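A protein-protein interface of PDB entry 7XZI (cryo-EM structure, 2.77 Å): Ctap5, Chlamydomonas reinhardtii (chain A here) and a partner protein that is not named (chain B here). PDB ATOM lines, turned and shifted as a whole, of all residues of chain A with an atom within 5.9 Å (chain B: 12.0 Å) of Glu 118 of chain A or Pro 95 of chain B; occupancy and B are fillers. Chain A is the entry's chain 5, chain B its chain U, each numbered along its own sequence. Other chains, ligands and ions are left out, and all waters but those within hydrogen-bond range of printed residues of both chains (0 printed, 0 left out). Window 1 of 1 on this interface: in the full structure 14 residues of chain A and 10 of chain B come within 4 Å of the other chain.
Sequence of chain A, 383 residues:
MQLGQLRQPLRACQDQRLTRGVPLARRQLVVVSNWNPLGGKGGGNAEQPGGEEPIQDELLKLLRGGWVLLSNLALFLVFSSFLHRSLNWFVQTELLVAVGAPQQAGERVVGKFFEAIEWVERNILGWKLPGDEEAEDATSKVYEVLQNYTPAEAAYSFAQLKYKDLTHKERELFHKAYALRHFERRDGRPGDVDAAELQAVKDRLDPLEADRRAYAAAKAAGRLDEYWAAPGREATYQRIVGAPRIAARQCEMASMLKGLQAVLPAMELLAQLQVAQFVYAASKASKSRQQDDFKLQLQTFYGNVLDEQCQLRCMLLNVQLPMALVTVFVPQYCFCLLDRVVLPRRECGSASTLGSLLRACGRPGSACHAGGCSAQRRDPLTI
The side-chain hydroxyl (OH) of Tyr 83 of chain B is in hydrogen-bond range of the backbone carbonyl oxygen (O) of Asn 123 of chain A.
The backbone NH (N) of Val 97 of chain B sits at hydrogen-bond distance from the side-chain carboxylate (OE2) of Glu 118 of chain A (2.9 Å).
O of Ile 96 of chain B sits close to OD1 of Asn 98 of chain B, at 2.8 Å.
ND2 of Asn 123 of chain A sits close to NE1 of Trp 119 of chain A (3.4 Å).
The side-chain hydroxyl of Thr 86 of chain B is in hydrogen-bond range of the backbone carbonyl oxygen of Tyr 83 of chain B, at 3.4 Å.
Ile 96 of chain B touches Phe 114 of chain A (O to CD1, 3.7 Å).
Phe 114 of chain A touches Val 97 of chain B.
Phe 114 of chain A touches Asn 98 of chain B (CZ to OD1, 3.97 Å).
Val 97 of chain B touches Glu 115 of chain A (CG2 to N, 3.8 Å).
CG of Glu 118 of chain A touches O of Pro 95 of chain B, at 3.9 Å.
Ile 96 of chain B touches Glu 118 of chain A.
Glu 121 of chain A touches Pro 95 of chain B.
Arg 122 of chain A touches Tyr 83 of chain B (O to OH, 3.9 Å).
CD1 of Ile 96 of chain B touches CD2 of Leu 129 of chain A (3.7 Å).
Phe 114 of chain A touches just these residues of chain B: Ile 96 (3.7 Å), Val 97 (3.5 Å) and Asn 98 (3.97 Å).
No residue of chain B comes within 4 Å of Ala 116 of chain A.
No residue of chain B comes within 4 Å of Ile 117 of chain A.
Glu 118 of chain A touches just these residues of chain B: Pro 95 (3.9 Å), Ile 96 (3.2 Å) and Val 97 (2.9 Å).
Glu 121 of chain A touches just one residue of chain B: Pro 95 (3.3 Å).
Of the printed residues of chain B, Arg 122 of chain A touches Tyr 83 (3.9 Å).
Printed residues of chain B within 4 Å of Leu 129 of chain A: Ile 96.
Of the printed residues of chain A, Tyr 83 of chain B touches Arg 122 and Asn 123.
Leu 89 of chain B touches none of the printed residues of chain A.
Gly 91 of chain B touches none of the printed residues of chain A.
Printed residues of chain A within 4 Å of Asn 98 of chain B: Phe 114.
The nearest residue of chain A that does not touch Pro 95 of chain B is Leu 129 of chain A (4.5 Å).
The nearest printed residue of chain A that does not touch Val 97 of chain B is Phe 113 of chain A (6.3 Å).
Of the 12 printed residues of chain A, 7 touch a printed residue of chain B.
Hydrophobic or aromatic side chains of chain A that line the printed part of chain B: Phe 114 and Leu 129.
Hydrophobic or aromatic side chains of chain B that line the printed part of chain A: Tyr 83, Pro 95, Ile 96 and Val 97.
Among the printed residues, 11 pairs touch across the chains.
Among the printed residues, no Asp or Glu carboxylate lies within 4 Å of a Lys or Arg side-chain nitrogen of the other chain.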
ATOM      1  N   PHE A 113      22.703  -8.233 -26.717  1.00  0.00           N
ATOM      2  CA  PHE A 113      23.754  -9.233 -26.533  1.00  0.00           C
ATOM      3  C   PHE A 113      23.615  -9.944 -25.187  1.00  0.00           C
ATOM      4  O   PHE A 113      23.725 -11.175 -25.105  1.00  0.00           O
ATOM      5  CB  PHE A 113      25.129  -8.577 -26.654  1.00  0.00           C
ATOM      6  CG  PHE A 113      26.274  -9.536 -26.498  1.00  0.00           C
ATOM      7  N   PHE A 114      23.361  -9.182 -24.121  1.00  0.00           N
ATOM      8  CA  PHE A 114      23.181  -9.776 -22.802  1.00  0.00           C
ATOM      9  C   PHE A 114      21.915 -10.617 -22.727  1.00  0.00           C
ATOM     10  O   PHE A 114      21.872 -11.590 -21.975  1.00  0.00           O
ATOM     11  CB  PHE A 114      23.161  -8.687 -21.730  1.00  0.00           C
ATOM     12  CG  PHE A 114      24.511  -8.380 -21.150  1.00  0.00           C
ATOM     13  CD1 PHE A 114      25.037  -9.166 -20.139  1.00  0.00           C
ATOM     14  CD2 PHE A 114      25.251  -7.303 -21.610  1.00  0.00           C
ATOM     15  CE1 PHE A 114      26.278  -8.886 -19.600  1.00  0.00           C
ATOM     16  CE2 PHE A 114      26.492  -7.019 -21.074  1.00  0.00           C
ATOM     17  CZ  PHE A 114      27.006  -7.811 -20.069  1.00  0.00           C
ATOM     18  N   GLU A 115      20.875 -10.257 -23.482  1.00  0.00           N
ATOM     19  CA  GLU A 115      19.683 -11.095 -23.552  1.00  0.00           C
ATOM     20  C   GLU A 115      19.993 -12.426 -24.223  1.00  0.00           C
ATOM     21  O   GLU A 115      19.493 -13.475 -23.798  1.00  0.00           O
ATOM     22  CB  GLU A 115      18.568 -10.362 -24.298  1.00  0.00           C
ATOM     23  N   ALA A 116      20.808 -12.401 -25.278  1.00  0.00           N
ATOM     24  CA  ALA A 116      21.257 -13.653 -25.883  1.00  0.00           C
ATOM     25  C   ALA A 116      22.044 -14.492 -24.882  1.00  0.00           C
ATOM     26  O   ALA A 116      21.845 -15.711 -24.782  1.00  0.00           O
ATOM     27  CB  ALA A 116      22.099 -13.365 -27.125  1.00  0.00           C
ATOM     28  N   ILE A 117      22.935 -13.850 -24.123  1.00  0.00           N
ATOM     29  CA  ILE A 117      23.707 -14.563 -23.106  1.00  0.00           C
ATOM     30  C   ILE A 117      22.784 -15.147 -22.040  1.00  0.00           C
ATOM     31  O   ILE A 117      22.983 -16.275 -21.571  1.00  0.00           O
ATOM     32  CB  ILE A 117      24.769 -13.631 -22.493  1.00  0.00           C
ATOM     33  CG1 ILE A 117      25.779 -13.198 -23.558  1.00  0.00           C
ATOM     34  CG2 ILE A 117      25.479 -14.312 -21.333  1.00  0.00           C
ATOM     35  CD1 ILE A 117      26.885 -12.312 -23.027  1.00  0.00           C
ATOM     36  N   GLU A 118      21.767 -14.383 -21.635  1.00  0.00           N
ATOM     37  CA  GLU A 118      20.810 -14.862 -20.645  1.00  0.00           C
ATOM     38  C   GLU A 118      20.031 -16.062 -21.161  1.00  0.00           C
ATOM     39  O   GLU A 118      19.763 -17.003 -20.410  1.00  0.00           O
ATOM     40  CB  GLU A 118      19.849 -13.741 -20.249  1.00  0.00           C
ATOM     41  CG  GLU A 118      20.433 -12.705 -19.309  1.00  0.00           C
ATOM     42  CD  GLU A 118      19.413 -11.661 -18.904  1.00  0.00           C
ATOM     43  OE1 GLU A 118      18.309 -11.650 -19.488  1.00  0.00           O
ATOM     44  OE2 GLU A 118      19.712 -10.854 -18.000  1.00  0.00           O
ATOM     45  N   TRP A 119      19.633 -16.034 -22.435  1.00  0.00           N
ATOM     46  CA  TRP A 119      18.954 -17.192 -23.008  1.00  0.00           C
ATOM     47  C   TRP A 119      19.870 -18.406 -23.015  1.00  0.00           C
ATOM     48  O   TRP A 119      19.435 -19.525 -22.718  1.00  0.00           O
ATOM     49  CB  TRP A 119      18.466 -16.886 -24.422  1.00  0.00           C
ATOM     50  CG  TRP A 119      17.558 -17.950 -24.974  1.00  0.00           C
ATOM     51  CD1 TRP A 119      16.195 -17.946 -24.965  1.00  0.00           C
ATOM     52  CD2 TRP A 119      17.951 -19.175 -25.606  1.00  0.00           C
ATOM     53  NE1 TRP A 119      15.712 -19.089 -25.555  1.00  0.00           N
ATOM     54  CE2 TRP A 119      16.770 -19.861 -25.957  1.00  0.00           C
ATOM     55  CE3 TRP A 119      19.184 -19.759 -25.913  1.00  0.00           C
ATOM     56  CZ2 TRP A 119      16.787 -21.099 -26.597  1.00  0.00           C
ATOM     57  CZ3 TRP A 119      19.198 -20.989 -26.547  1.00  0.00           C
ATOM     58  CH2 TRP A 119      18.007 -21.645 -26.882  1.00  0.00           C
ATOM     59  N   VAL A 120      21.146 -18.201 -23.355  1.00  0.00           N
ATOM     60  CA  VAL A 120      22.104 -19.304 -23.332  1.00  0.00           C
ATOM     61  C   VAL A 120      22.209 -19.890 -21.929  1.00  0.00           C
ATOM     62  O   VAL A 120      22.220 -21.114 -21.748  1.00  0.00           O
ATOM     63  CB  VAL A 120      23.475 -18.834 -23.855  1.00  0.00           C
ATOM     64  CG1 VAL A 120      24.532 -19.898 -23.608  1.00  0.00           C
ATOM     65  CG2 VAL A 120      23.389 -18.504 -25.335  1.00  0.00           C
ATOM     66  N   GLU A 121      22.287 -19.027 -20.915  1.00  0.00           N
ATOM     67  CA  GLU A 121      22.369 -19.509 -19.538  1.00  0.00           C
ATOM     68  C   GLU A 121      21.097 -20.244 -19.123  1.00  0.00           C
ATOM     69  O   GLU A 121      21.161 -21.295 -18.477  1.00  0.00           O
ATOM     70  CB  GLU A 121      22.642 -18.343 -18.586  1.00  0.00           C
ATOM     71  CG  GLU A 121      23.961 -17.630 -18.826  1.00  0.00           C
ATOM     72  CD  GLU A 121      24.214 -16.518 -17.826  1.00  0.00           C
ATOM     73  OE1 GLU A 121      23.523 -16.483 -16.786  1.00  0.00           O
ATOM     74  OE2 GLU A 121      25.101 -15.677 -18.082  1.00  0.00           O
ATOM     75  N   ARG A 122      19.933 -19.701 -19.481  1.00  0.00           N
ATOM     76  CA  ARG A 122      18.668 -20.201 -18.956  1.00  0.00           C
ATOM     77  C   ARG A 122      18.220 -21.490 -19.636  1.00  0.00           C
ATOM     78  O   ARG A 122      17.696 -22.392 -18.972  1.00  0.00           O
ATOM     79  CB  ARG A 122      17.596 -19.119 -19.096  1.00  0.00           C
ATOM     80  CG  ARG A 122      16.291 -19.416 -18.385  1.00  0.00           C
ATOM     81  CD  ARG A 122      15.654 -18.122 -17.910  1.00  0.00           C
ATOM     82  NE  ARG A 122      15.702 -17.092 -18.937  1.00  0.00           N
ATOM     83  CZ  ARG A 122      15.436 -15.807 -18.729  1.00  0.00           C
ATOM     84  NH1 ARG A 122      15.100 -15.357 -17.531  1.00  0.00           N
ATOM     85  NH2 ARG A 122      15.513 -14.955 -19.745  1.00  0.00           N
ATOM     86  N   ASN A 123      18.410 -21.601 -20.951  1.00  0.00           N
ATOM     87  CA  ASN A 123      17.911 -22.749 -21.702  1.00  0.00           C
ATOM     88  C   ASN A 123      18.979 -23.808 -21.949  1.00  0.00           C
ATOM     89  O   ASN A 123      18.757 -24.988 -21.658  1.00  0.00           O
ATOM     90  CB  ASN A 123      17.315 -22.288 -23.037  1.00  0.00           C
ATOM     91  CG  ASN A 123      15.865 -21.862 -22.910  1.00  0.00           C
ATOM     92  OD1 ASN A 123      14.952 -22.659 -23.126  1.00  0.00           O
ATOM     93  ND2 ASN A 123      15.645 -20.600 -22.559  1.00  0.00           N
ATOM     94  N   LEU A 129      17.569 -17.781 -12.936  1.00  0.00           N
ATOM     95  CA  LEU A 129      18.011 -16.409 -12.753  1.00  0.00           C
ATOM     96  C   LEU A 129      17.120 -15.712 -11.735  1.00  0.00           C
ATOM     97  O   LEU A 129      15.952 -16.079 -11.572  1.00  0.00           O
ATOM     98  CB  LEU A 129      17.979 -15.630 -14.078  1.00  0.00           C
ATOM     99  CG  LEU A 129      19.156 -15.763 -15.052  1.00  0.00           C
ATOM    100  CD1 LEU A 129      19.245 -17.154 -15.662  1.00  0.00           C
ATOM    101  CD2 LEU A 129      19.060 -14.708 -16.143  1.00  0.00           C
ATOM    102  N   TYR B  83      21.034 -31.469 -17.624  1.00  0.00           N
ATOM    103  CA  TYR B  83      20.882 -30.456 -16.586  1.00  0.00           C
ATOM    104  C   TYR B  83      21.647 -30.806 -15.318  1.00  0.00           C
ATOM    105  O   TYR B  83      22.162 -29.907 -14.653  1.00  0.00           O
ATOM    106  CB  TYR B  83      19.403 -30.227 -16.278  1.00  0.00           C
ATOM    107  CG  TYR B  83      18.778 -29.164 -17.156  1.00  0.00           C
ATOM    108  CD1 TYR B  83      19.559 -28.423 -18.034  1.00  0.00           C
ATOM    109  CD2 TYR B  83      17.418 -28.896 -17.103  1.00  0.00           C
ATOM    110  CE1 TYR B  83      19.003 -27.450 -18.839  1.00  0.00           C
ATOM    111  CE2 TYR B  83      16.851 -27.922 -17.907  1.00  0.00           C
ATOM    112  CZ  TYR B  83      17.649 -27.202 -18.772  1.00  0.00           C
ATOM    113  OH  TYR B  83      17.096 -26.232 -19.574  1.00  0.00           O
ATOM    114  N   THR B  86      25.221 -29.775 -16.149  1.00  0.00           N
ATOM    115  CA  THR B  86      25.395 -28.332 -16.259  1.00  0.00           C
ATOM    116  C   THR B  86      24.986 -27.573 -15.002  1.00  0.00           C
ATOM    117  O   THR B  86      25.240 -26.366 -14.918  1.00  0.00           O
ATOM    118  CB  THR B  86      24.603 -27.793 -17.454  1.00  0.00           C
ATOM    119  OG1 THR B  86      23.216 -28.111 -17.292  1.00  0.00           O
ATOM    120  CG2 THR B  86      25.109 -28.413 -18.747  1.00  0.00           C
ATOM    121  N   LEU B  89      27.760 -27.410 -11.373  1.00  0.00           N
ATOM    122  CA  LEU B  89      28.298 -26.079 -11.121  1.00  0.00           C
ATOM    123  C   LEU B  89      27.172 -25.186 -10.618  1.00  0.00           C
ATOM    124  O   LEU B  89      26.133 -25.082 -11.285  1.00  0.00           O
ATOM    125  CB  LEU B  89      28.916 -25.489 -12.387  1.00  0.00           C
ATOM    126  CG  LEU B  89      30.036 -26.236 -13.118  1.00  0.00           C
ATOM    127  CD1 LEU B  89      29.485 -27.314 -14.045  1.00  0.00           C
ATOM    128  CD2 LEU B  89      30.905 -25.259 -13.896  1.00  0.00           C
ATOM    129  N   PRO B  90      27.318 -24.531  -9.467  1.00  0.00           N
ATOM    130  CA  PRO B  90      26.238 -23.669  -8.968  1.00  0.00           C
ATOM    131  C   PRO B  90      26.091 -22.395  -9.785  1.00  0.00           C
ATOM    132  O   PRO B  90      26.804 -22.200 -10.774  1.00  0.00           O
ATOM    133  CB  PRO B  90      26.668 -23.368  -7.528  1.00  0.00           C
ATOM    134  CG  PRO B  90      28.157 -23.468  -7.565  1.00  0.00           C
ATOM    135  CD  PRO B  90      28.470 -24.564  -8.550  1.00  0.00           C
ATOM    136  N   GLY B  91      25.163 -21.528  -9.387  1.00  0.00           N
ATOM    137  CA  GLY B  91      24.980 -20.259 -10.064  1.00  0.00           C
ATOM    138  C   GLY B  91      26.229 -19.404 -10.037  1.00  0.00           C
ATOM    139  O   GLY B  91      26.620 -18.898  -8.981  1.00  0.00           O
ATOM    140  N   HIS B  92      26.866 -19.238 -11.195  1.00  0.00           N
ATOM    141  CA  HIS B  92      28.122 -18.494 -11.293  1.00  0.00           C
ATOM    142  C   HIS B  92      27.852 -16.997 -11.470  1.00  0.00           C
ATOM    143  O   HIS B  92      28.136 -16.397 -12.507  1.00  0.00           O
ATOM    144  CB  HIS B  92      28.975 -19.047 -12.428  1.00  0.00           C
ATOM    145  CG  HIS B  92      29.527 -20.412 -12.158  1.00  0.00           C
ATOM    146  ND1 HIS B  92      29.217 -21.130 -11.023  1.00  0.00           N
ATOM    147  CD2 HIS B  92      30.374 -21.190 -12.874  1.00  0.00           C
ATOM    148  CE1 HIS B  92      29.846 -22.290 -11.051  1.00  0.00           C
ATOM    149  NE2 HIS B  92      30.555 -22.352 -12.164  1.00  0.00           N
ATOM    150  N   ASP B  93      27.255 -16.417 -10.426  1.00  0.00           N
ATOM    151  CA  ASP B  93      27.015 -14.982 -10.289  1.00  0.00           C
ATOM    152  C   ASP B  93      25.911 -14.488 -11.218  1.00  0.00           C
ATOM    153  O   ASP B  93      25.486 -13.333 -11.112  1.00  0.00           O
ATOM    154  CB  ASP B  93      28.303 -14.186 -10.530  1.00  0.00           C
ATOM    155  N   ASN B  94      25.431 -15.358 -12.116  1.00  0.00           N
ATOM    156  CA  ASN B  94      24.258 -15.112 -12.950  1.00  0.00           C
ATOM    157  C   ASN B  94      24.300 -13.744 -13.624  1.00  0.00           C
ATOM    158  O   ASN B  94      23.588 -12.829 -13.194  1.00  0.00           O
ATOM    159  CB  ASN B  94      22.983 -15.241 -12.115  1.00  0.00           C
ATOM    160  CG  ASN B  94      22.874 -16.584 -11.424  1.00  0.00           C
ATOM    161  OD1 ASN B  94      22.629 -16.658 -10.219  1.00  0.00           O
ATOM    162  ND2 ASN B  94      23.060 -17.658 -12.184  1.00  0.00           N
ATOM    163  N   PRO B  95      25.135 -13.549 -14.646  1.00  0.00           N
ATOM    164  CA  PRO B  95      25.181 -12.243 -15.318  1.00  0.00           C
ATOM    165  C   PRO B  95      23.815 -11.839 -15.858  1.00  0.00           C
ATOM    166  O   PRO B  95      23.078 -12.655 -16.414  1.00  0.00           O
ATOM    167  CB  PRO B  95      26.193 -12.463 -16.449  1.00  0.00           C
ATOM    168  CG  PRO B  95      27.047 -13.592 -15.973  1.00  0.00           C
ATOM    169  CD  PRO B  95      26.128 -14.489 -15.195  1.00  0.00           C
ATOM    170  N   ILE B  96      23.487 -10.556 -15.691  1.00  0.00           N
ATOM    171  CA  ILE B  96      22.187 -10.009 -16.052  1.00  0.00           C
ATOM    172  C   ILE B  96      22.404  -8.805 -16.959  1.00  0.00           C
ATOM    173  O   ILE B  96      23.469  -8.183 -16.962  1.00  0.00           O
ATOM    174  CB  ILE B  96      21.359  -9.607 -14.803  1.00  0.00           C
ATOM    175  CG1 ILE B  96      21.361 -10.729 -13.767  1.00  0.00           C
ATOM    176  CG2 ILE B  96      19.916  -9.285 -15.168  1.00  0.00           C
ATOM    177  CD1 ILE B  96      20.637 -11.977 -14.219  1.00  0.00           C
ATOM    178  N   VAL B  97      21.377  -8.489 -17.751  1.00  0.00           N
ATOM    179  CA  VAL B  97      21.409  -7.292 -18.587  1.00  0.00           C
ATOM    180  C   VAL B  97      21.529  -6.069 -17.691  1.00  0.00           C
ATOM    181  O   VAL B  97      20.703  -5.853 -16.796  1.00  0.00           O
ATOM    182  CB  VAL B  97      20.159  -7.213 -19.468  1.00  0.00           C
ATOM    183  CG1 VAL B  97      20.253  -6.028 -20.418  1.00  0.00           C
ATOM    184  CG2 VAL B  97      19.957  -8.509 -20.236  1.00  0.00           C
ATOM    185  N   ASN B  98      22.557  -5.260 -17.927  1.00  0.00           N
ATOM    186  CA  ASN B  98      22.754  -4.050 -17.139  1.00  0.00           C
ATOM    187  C   ASN B  98      21.806  -2.942 -17.595  1.00  0.00           C
ATOM    188  O   ASN B  98      21.162  -2.308 -16.750  1.00  0.00           O
ATOM    189  CB  ASN B  98      24.212  -3.585 -17.207  1.00  0.00           C
ATOM    190  CG  ASN B  98      25.193  -4.700 -16.911  1.00  0.00           C
ATOM    191  OD1 ASN B  98      24.972  -5.852 -17.284  1.00  0.00           O
ATOM    192  ND2 ASN B  98      26.283  -4.366 -16.230  1.00  0.00           N
ATOM    193  N   PRO B  99      21.679  -2.664 -18.910  1.00  0.00           N
ATOM    194  CA  PRO B  99      20.703  -1.628 -19.262  1.00  0.00           C
ATOM    195  C   PRO B  99      19.264  -2.138 -19.262  1.00  0.00           C
ATOM    196  O   PRO B  99      18.925  -3.014 -18.466  1.00  0.00           O
ATOM    197  CB  PRO B  99      21.123  -1.210 -20.680  1.00  0.00           C
ATOM    198  CG  PRO B  99      22.485  -1.805 -20.893  1.00  0.00           C
ATOM    199  CD  PRO B  99      22.490  -3.051 -20.078  1.00  0.00           C
